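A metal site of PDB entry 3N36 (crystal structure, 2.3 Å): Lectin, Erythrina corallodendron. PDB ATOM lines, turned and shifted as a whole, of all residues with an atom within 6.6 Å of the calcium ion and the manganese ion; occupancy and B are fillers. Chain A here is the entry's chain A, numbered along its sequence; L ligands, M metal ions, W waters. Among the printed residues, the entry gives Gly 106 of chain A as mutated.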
ATOM      1  N   ASP A  89      -9.009 -20.160 -17.888  1.00  0.00           N
ATOM      2  CA  ASP A  89      -8.876 -19.087 -18.883  1.00  0.00           C
ATOM      3  C   ASP A  89     -10.237 -18.440 -19.149  1.00  0.00           C
ATOM      4  O   ASP A  89     -10.306 -17.302 -19.623  1.00  0.00           O
ATOM      5  CB  ASP A  89      -8.347 -19.647 -20.199  1.00  0.00           C
ATOM      6  CG  ASP A  89      -6.834 -19.631 -20.265  1.00  0.00           C
ATOM      7  OD1 ASP A  89      -6.264 -18.529 -20.342  1.00  0.00           O
ATOM      8  OD2 ASP A  89      -6.235 -20.727 -20.249  1.00  0.00           O
ATOM      9  N   GLY A 106      -6.641 -23.308 -23.637  1.00  0.00           N
ATOM     10  CA  GLY A 106      -6.018 -22.164 -22.988  1.00  0.00           C
ATOM     11  C   GLY A 106      -6.688 -20.840 -23.333  1.00  0.00           C
ATOM     12  O   GLY A 106      -7.915 -20.751 -23.366  1.00  0.00           O
ATOM     13  N   GLY A 107      -5.879 -19.815 -23.578  1.00  0.00           N
ATOM     14  CA  GLY A 107      -6.418 -18.507 -23.903  1.00  0.00           C
ATOM     15  C   GLY A 107      -7.274 -18.431 -25.168  1.00  0.00           C
ATOM     16  O   GLY A 107      -7.893 -17.409 -25.436  1.00  0.00           O
ATOM     17  N   TYR A 108      -7.302 -19.503 -25.955  1.00  0.00           N
ATOM     18  CA  TYR A 108      -8.091 -19.505 -27.194  1.00  0.00           C
ATOM     19  C   TYR A 108      -9.486 -20.043 -26.939  1.00  0.00           C
ATOM     20  O   TYR A 108     -10.302 -20.127 -27.855  1.00  0.00           O
ATOM     21  CB  TYR A 108      -7.375 -20.310 -28.275  1.00  0.00           C
ATOM     22  CG  TYR A 108      -6.038 -19.720 -28.653  1.00  0.00           C
ATOM     23  CD1 TYR A 108      -5.957 -18.428 -29.167  1.00  0.00           C
ATOM     24  CD2 TYR A 108      -4.851 -20.419 -28.430  1.00  0.00           C
ATOM     25  CE1 TYR A 108      -4.736 -17.851 -29.463  1.00  0.00           C
ATOM     26  CE2 TYR A 108      -3.621 -19.845 -28.726  1.00  0.00           C
ATOM     27  CZ  TYR A 108      -3.563 -18.559 -29.236  1.00  0.00           C
ATOM     28  OH  TYR A 108      -2.345 -17.984 -29.500  1.00  0.00           O
ATOM     29  N   LEU A 109      -9.740 -20.396 -25.686  1.00  0.00           N
ATOM     30  CA  LEU A 109     -11.037 -20.886 -25.228  1.00  0.00           C
ATOM     31  C   LEU A 109     -11.697 -22.037 -25.986  1.00  0.00           C
ATOM     32  O   LEU A 109     -12.918 -22.219 -25.906  1.00  0.00           O
ATOM     33  CB  LEU A 109     -12.017 -19.706 -25.145  1.00  0.00           C
ATOM     34  CG  LEU A 109     -11.480 -18.505 -24.337  1.00  0.00           C
ATOM     35  CD1 LEU A 109     -12.501 -17.374 -24.368  1.00  0.00           C
ATOM     36  CD2 LEU A 109     -11.171 -18.942 -22.907  1.00  0.00           C
ATOM     37  N   GLU A 127     -17.352 -13.987 -24.808  1.00  0.00           N
ATOM     38  CA  GLU A 127     -16.500 -14.588 -23.793  1.00  0.00           C
ATOM     39  C   GLU A 127     -16.606 -13.985 -22.409  1.00  0.00           C
ATOM     40  O   GLU A 127     -17.104 -12.860 -22.207  1.00  0.00           O
ATOM     41  CB  GLU A 127     -15.044 -14.531 -24.236  1.00  0.00           C
ATOM     42  CG  GLU A 127     -14.591 -13.076 -24.406  1.00  0.00           C
ATOM     43  CD  GLU A 127     -13.099 -12.901 -24.631  1.00  0.00           C
ATOM     44  OE1 GLU A 127     -12.504 -13.633 -25.413  1.00  0.00           O
ATOM     45  OE2 GLU A 127     -12.524 -12.020 -23.974  1.00  0.00           O
ATOM     46  N   ASP A 129     -13.894 -13.878 -19.928  1.00  0.00           N
ATOM     47  CA  ASP A 129     -12.448 -14.057 -19.821  1.00  0.00           C
ATOM     48  C   ASP A 129     -11.830 -13.785 -18.456  1.00  0.00           C
ATOM     49  O   ASP A 129     -11.856 -12.655 -17.985  1.00  0.00           O
ATOM     50  CB  ASP A 129     -11.772 -13.134 -20.833  1.00  0.00           C
ATOM     51  CG  ASP A 129     -10.429 -13.585 -21.235  1.00  0.00           C
ATOM     52  OD1 ASP A 129      -9.733 -14.180 -20.403  1.00  0.00           O
ATOM     53  OD2 ASP A 129     -10.090 -13.309 -22.403  1.00  0.00           O
ATOM     54  N   THR A 130     -11.171 -14.802 -17.949  1.00  0.00           N
ATOM     55  CA  THR A 130     -10.565 -14.666 -16.629  1.00  0.00           C
ATOM     56  C   THR A 130      -9.039 -14.497 -16.588  1.00  0.00           C
ATOM     57  O   THR A 130      -8.480 -14.269 -15.513  1.00  0.00           O
ATOM     58  CB  THR A 130     -10.943 -15.860 -15.752  1.00  0.00           C
ATOM     59  OG1 THR A 130     -10.498 -17.068 -16.390  1.00  0.00           O
ATOM     60  CG2 THR A 130     -12.456 -15.915 -15.549  1.00  0.00           C
ATOM     61  N   PHE A 131      -8.355 -14.603 -17.728  1.00  0.00           N
ATOM     62  CA  PHE A 131      -6.901 -14.435 -17.735  1.00  0.00           C
ATOM     63  C   PHE A 131      -6.493 -13.397 -18.743  1.00  0.00           C
ATOM     64  O   PHE A 131      -6.986 -13.409 -19.861  1.00  0.00           O
ATOM     65  CB  PHE A 131      -6.198 -15.756 -18.049  1.00  0.00           C
ATOM     66  CG  PHE A 131      -4.687 -15.662 -18.008  1.00  0.00           C
ATOM     67  CD1 PHE A 131      -4.003 -15.786 -16.796  1.00  0.00           C
ATOM     68  CD2 PHE A 131      -3.956 -15.444 -19.164  1.00  0.00           C
ATOM     69  CE1 PHE A 131      -2.603 -15.673 -16.747  1.00  0.00           C
ATOM     70  CE2 PHE A 131      -2.547 -15.339 -19.128  1.00  0.00           C
ATOM     71  CZ  PHE A 131      -1.874 -15.464 -17.908  1.00  0.00           C
ATOM     72  N   SER A 132      -5.587 -12.499 -18.374  1.00  0.00           N
ATOM     73  CA  SER A 132      -5.161 -11.451 -19.288  1.00  0.00           C
ATOM     74  C   SER A 132      -4.010 -11.886 -20.225  1.00  0.00           C
ATOM     75  O   SER A 132      -2.850 -11.850 -19.817  1.00  0.00           O
ATOM     76  CB  SER A 132      -4.729 -10.220 -18.500  1.00  0.00           C
ATOM     77  OG  SER A 132      -4.319  -9.178 -19.365  1.00  0.00           O
ATOM     78  N   ASN A 133      -4.344 -12.290 -21.444  1.00  0.00           N
ATOM     79  CA  ASN A 133      -3.336 -12.688 -22.438  1.00  0.00           C
ATOM     80  C   ASN A 133      -2.765 -11.444 -23.104  1.00  0.00           C
ATOM     81  O   ASN A 133      -3.252 -10.345 -22.878  1.00  0.00           O
ATOM     82  CB  ASN A 133      -3.932 -13.586 -23.521  1.00  0.00           C
ATOM     83  CG  ASN A 133      -4.184 -15.011 -23.027  1.00  0.00           C
ATOM     84  OD1 ASN A 133      -5.268 -15.349 -22.621  1.00  0.00           O
ATOM     85  ND2 ASN A 133      -3.160 -15.834 -23.071  1.00  0.00           N
ATOM     86  N   TRP A 135      -3.062 -10.263 -26.053  1.00  0.00           N
ATOM     87  CA  TRP A 135      -4.003  -9.552 -26.899  1.00  0.00           C
ATOM     88  C   TRP A 135      -5.146  -8.987 -26.052  1.00  0.00           C
ATOM     89  O   TRP A 135      -6.044  -8.334 -26.574  1.00  0.00           O
ATOM     90  CB  TRP A 135      -4.589 -10.507 -27.937  1.00  0.00           C
ATOM     91  CG  TRP A 135      -5.200 -11.750 -27.322  1.00  0.00           C
ATOM     92  CD1 TRP A 135      -6.436 -11.885 -26.757  1.00  0.00           C
ATOM     93  CD2 TRP A 135      -4.581 -13.051 -27.219  1.00  0.00           C
ATOM     94  NE1 TRP A 135      -6.635 -13.165 -26.316  1.00  0.00           N
ATOM     95  CE2 TRP A 135      -5.505 -13.905 -26.591  1.00  0.00           C
ATOM     96  CE3 TRP A 135      -3.333 -13.563 -27.599  1.00  0.00           C
ATOM     97  CZ2 TRP A 135      -5.229 -15.254 -26.323  1.00  0.00           C
ATOM     98  CZ3 TRP A 135      -3.054 -14.899 -27.337  1.00  0.00           C
ATOM     99  CH2 TRP A 135      -3.992 -15.735 -26.715  1.00  0.00           C
ATOM    100  N   ASP A 136      -5.107  -9.249 -24.749  1.00  0.00           N
ATOM    101  CA  ASP A 136      -6.166  -8.801 -23.854  1.00  0.00           C
ATOM    102  C   ASP A 136      -5.977  -7.458 -23.147  1.00  0.00           C
ATOM    103  O   ASP A 136      -4.867  -6.964 -22.984  1.00  0.00           O
ATOM    104  CB  ASP A 136      -6.400  -9.838 -22.745  1.00  0.00           C
ATOM    105  CG  ASP A 136      -7.246 -11.007 -23.186  1.00  0.00           C
ATOM    106  OD1 ASP A 136      -8.100 -10.858 -24.084  1.00  0.00           O
ATOM    107  OD2 ASP A 136      -7.056 -12.081 -22.609  1.00  0.00           O
ATOM    108  N   PRO A 137      -7.106  -6.843 -22.747  1.00  0.00           N
ATOM    109  CA  PRO A 137      -6.996  -5.575 -22.019  1.00  0.00           C
ATOM    110  C   PRO A 137      -6.460  -6.077 -20.679  1.00  0.00           C
ATOM    111  O   PRO A 137      -6.627  -7.251 -20.343  1.00  0.00           O
ATOM    112  CB  PRO A 137      -8.444  -5.086 -21.928  1.00  0.00           C
ATOM    113  CG  PRO A 137      -9.261  -6.356 -22.043  1.00  0.00           C
ATOM    114  CD  PRO A 137      -8.500  -7.123 -23.111  1.00  0.00           C
ATOM    115  N   VAL A 140      -9.199  -8.138 -15.826  1.00  0.00           N
ATOM    116  CA  VAL A 140      -9.857  -9.431 -15.896  1.00  0.00           C
ATOM    117  C   VAL A 140     -10.569  -9.623 -14.561  1.00  0.00           C
ATOM    118  O   VAL A 140     -10.107  -9.132 -13.545  1.00  0.00           O
ATOM    119  CB  VAL A 140      -8.877 -10.605 -16.119  1.00  0.00           C
ATOM    120  CG1 VAL A 140      -8.412 -10.633 -17.557  1.00  0.00           C
ATOM    121  CG2 VAL A 140      -7.696 -10.498 -15.155  1.00  0.00           C
ATOM    122  N   HIS A 142     -13.304 -10.076 -17.870  1.00  0.00           N
ATOM    123  CA  HIS A 142     -13.998  -9.138 -18.732  1.00  0.00           C
ATOM    124  C   HIS A 142     -14.884  -9.901 -19.687  1.00  0.00           C
ATOM    125  O   HIS A 142     -14.634 -11.060 -19.995  1.00  0.00           O
ATOM    126  CB  HIS A 142     -13.027  -8.238 -19.519  1.00  0.00           C
ATOM    127  CG  HIS A 142     -12.062  -8.988 -20.387  1.00  0.00           C
ATOM    128  ND1 HIS A 142     -10.802  -9.341 -19.970  1.00  0.00           N
ATOM    129  CD2 HIS A 142     -12.178  -9.446 -21.660  1.00  0.00           C
ATOM    130  CE1 HIS A 142     -10.180  -9.998 -20.935  1.00  0.00           C
ATOM    131  NE2 HIS A 142     -10.995 -10.070 -21.977  1.00  0.00           N
ATOM    132  N   ILE A 143     -15.943  -9.239 -20.118  1.00  0.00           N
ATOM    133  CA  ILE A 143     -16.862  -9.820 -21.074  1.00  0.00           C
ATOM    134  C   ILE A 143     -16.304  -9.333 -22.401  1.00  0.00           C
ATOM    135  O   ILE A 143     -15.737  -8.240 -22.482  1.00  0.00           O
ATOM    136  CB  ILE A 143     -18.284  -9.241 -20.921  1.00  0.00           C
ATOM    137  CG1 ILE A 143     -18.752  -9.378 -19.473  1.00  0.00           C
ATOM    138  CG2 ILE A 143     -19.231  -9.969 -21.887  1.00  0.00           C
ATOM    139  CD1 ILE A 143     -20.024  -8.617 -19.196  1.00  0.00           C
ATOM    140  N   GLY A 144     -16.448 -10.139 -23.445  1.00  0.00           N
ATOM    141  CA  GLY A 144     -15.946  -9.715 -24.719  1.00  0.00           C
ATOM    142  C   GLY A 144     -16.755 -10.227 -25.878  1.00  0.00           C
ATOM    143  O   GLY A 144     -17.312 -11.325 -25.819  1.00  0.00           O
ATOM    144  N   ASP A 146     -16.363 -11.410 -29.499  1.00  0.00           N
ATOM    145  CA  ASP A 146     -15.344 -11.888 -30.424  1.00  0.00           C
ATOM    146  C   ASP A 146     -15.925 -12.145 -31.798  1.00  0.00           C
ATOM    147  O   ASP A 146     -16.896 -12.880 -31.952  1.00  0.00           O
ATOM    148  CB  ASP A 146     -14.704 -13.172 -29.895  1.00  0.00           C
ATOM    149  CG  ASP A 146     -14.079 -13.001 -28.514  1.00  0.00           C
ATOM    150  OD1 ASP A 146     -13.871 -11.847 -28.106  1.00  0.00           O
ATOM    151  OD2 ASP A 146     -13.791 -14.020 -27.851  1.00  0.00           O
ATOM    152  N   ILE A 150      -9.807 -13.886 -31.325  1.00  0.00           N
ATOM    153  CA  ILE A 150      -9.825 -13.973 -29.866  1.00  0.00           C
ATOM    154  C   ILE A 150      -9.650 -12.549 -29.326  1.00  0.00           C
ATOM    155  O   ILE A 150     -10.010 -12.242 -28.196  1.00  0.00           O
ATOM    156  CB  ILE A 150      -8.695 -14.910 -29.355  1.00  0.00           C
ATOM    157  CG1 ILE A 150      -8.846 -15.128 -27.842  1.00  0.00           C
ATOM    158  CG2 ILE A 150      -7.326 -14.339 -29.689  1.00  0.00           C
ATOM    159  CD1 ILE A 150     -10.138 -15.802 -27.434  1.00  0.00           C
ATOM    160  N   ARG A 151      -9.096 -11.669 -30.160  1.00  0.00           N
ATOM    161  CA  ARG A 151      -8.926 -10.262 -29.803  1.00  0.00           C
ATOM    162  C   ARG A 151     -10.294  -9.595 -30.009  1.00  0.00           C
ATOM    163  O   ARG A 151     -10.729  -9.377 -31.146  1.00  0.00           O
ATOM    164  CB  ARG A 151      -7.865  -9.618 -30.717  1.00  0.00           C
ATOM    165  CG  ARG A 151      -7.613  -8.140 -30.425  1.00  0.00           C
ATOM    166  CD  ARG A 151      -6.588  -7.512 -31.352  1.00  0.00           C
ATOM    167  NE  ARG A 151      -5.209  -7.627 -30.862  1.00  0.00           N
ATOM    168  CZ  ARG A 151      -4.407  -8.668 -31.079  1.00  0.00           C
ATOM    169  NH1 ARG A 151      -4.822  -9.712 -31.789  1.00  0.00           N
ATOM    170  NH2 ARG A 151      -3.169  -8.668 -30.571  1.00  0.00           N
ATOM    171  N   SER A 152     -10.963  -9.270 -28.910  1.00  0.00           N
ATOM    172  CA  SER A 152     -12.309  -8.690 -28.938  1.00  0.00           C
ATOM    173  C   SER A 152     -12.458  -7.328 -29.624  1.00  0.00           C
ATOM    174  O   SER A 152     -11.573  -6.486 -29.544  1.00  0.00           O
ATOM    175  CB  SER A 152     -12.841  -8.549 -27.503  1.00  0.00           C
ATOM    176  OG  SER A 152     -12.861  -9.787 -26.824  1.00  0.00           O
ATOM    177  N   THR A 155     -14.831  -4.938 -25.168  1.00  0.00           N
ATOM    178  CA  THR A 155     -14.803  -5.604 -23.872  1.00  0.00           C
ATOM    179  C   THR A 155     -15.403  -4.762 -22.753  1.00  0.00           C
ATOM    180  O   THR A 155     -15.433  -3.529 -22.832  1.00  0.00           O
ATOM    181  CB  THR A 155     -13.364  -5.961 -23.443  1.00  0.00           C
ATOM    182  OG1 THR A 155     -12.584  -4.771 -23.357  1.00  0.00           O
ATOM    183  CG2 THR A 155     -12.731  -6.931 -24.431  1.00  0.00           C
HETATM  184  C1  LIG L   1      -0.442 -19.823 -20.625  1.00  0.00           C
HETATM  185  C2  LIG L   1      -1.621 -19.642 -21.574  1.00  0.00           C
HETATM  186  C3  LIG L   1      -2.724 -18.809 -20.919  1.00  0.00           C
HETATM  187  C4  LIG L   1      -3.053 -19.327 -19.528  1.00  0.00           C
HETATM  188  C5  LIG L   1      -1.788 -19.526 -18.700  1.00  0.00           C
HETATM  189  C6  LIG L   1      -2.108 -20.115 -17.334  1.00  0.00           C
HETATM  190  O1  LIG L   1       0.155 -18.545 -20.355  1.00  0.00           O
HETATM  191  O2  LIG L   1      -1.176 -18.996 -22.773  1.00  0.00           O
HETATM  192  O3  LIG L   1      -3.892 -18.851 -21.735  1.00  0.00           O
HETATM  193  O4  LIG L   1      -3.746 -20.577 -19.643  1.00  0.00           O
HETATM  194  O5  LIG L   1      -0.896 -20.398 -19.401  1.00  0.00           O
HETATM  195  O6  LIG L   1      -0.978 -19.958 -16.469  1.00  0.00           O
HETATM  196 CA    CA M   1      -7.610 -14.330 -22.105  1.00  0.00          CA
HETATM  197 MN    MN M   2     -10.415 -11.515 -23.817  1.00  0.00          MN
HETATM  198  O   HOH W   1      -8.530 -14.927 -24.456  1.00  0.00           O
HETATM  199  O   HOH W   2      -7.982 -16.672 -20.991  1.00  0.00           O
HETATM  200  O   HOH W   3      -9.846 -12.894 -25.644  1.00  0.00           O
HETATM  201  O   HOH W   4     -10.717  -9.571 -25.124  1.00  0.00           O
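An oxygen (O4) of the ligand sits at hydrogen-bond distance from the side-chain carboxylate of Asp 89 (2.6 Å).
N of Gly 107 sits at hydrogen-bond distance from O3 of the ligand, 2.9 Å away.
The side-chain amide nitrogen (ND2) of Asn 133 is in hydrogen-bond range of an oxygen (O3) of the ligand (3.4 Å).
O of Gly 144 is in hydrogen-bond range of N of Glu 127 (2.8 Å).
The nearest printed residue that does not touch the calcium ion is Trp 135 (4.5 Å).
Of the 23 residues printed, 4 come within 4 Å of the manganese ion.
The calcium ion is bound by OD2 of Asp 136 (2.4 Å), O of Phe 131 (2.5 Å), water W1 (2.6 Å), OD1 of Asn 133 (2.6 Å), water W2 (2.6 Å), OD2 of Asp 129 (2.7 Å) and OD1 of Asp 129 (2.7 Å).
The calcium ion has seven donor atoms within binding distance.
The manganese ion is bound by the side-chain carboxylate (OE2) of Glu 127, 2.2 Å away.
The manganese ion is bound by OD2 of Asp 129 (2.3 Å).
Water W3 binds the manganese ion, 2.4 Å away.
The manganese ion is bound by water W4 (2.4 Å).
A ring nitrogen (NE2) of His 142 binds the manganese ion, 2.4 Å away.
OD1 of Asp 136 binds the manganese ion, at 2.4 Å.
Water W1 bridges the backbone carbonyl oxygen (O) of Gly 107 (2.7 Å) and the indole nitrogen (NE1) of Trp 135 (3.2 Å).
Water W3 lies within hydrogen-bond range of the backbone carbonyl oxygen of Ile 150, the side-chain carboxylate of Glu 127 and the indole nitrogen of Trp 135.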
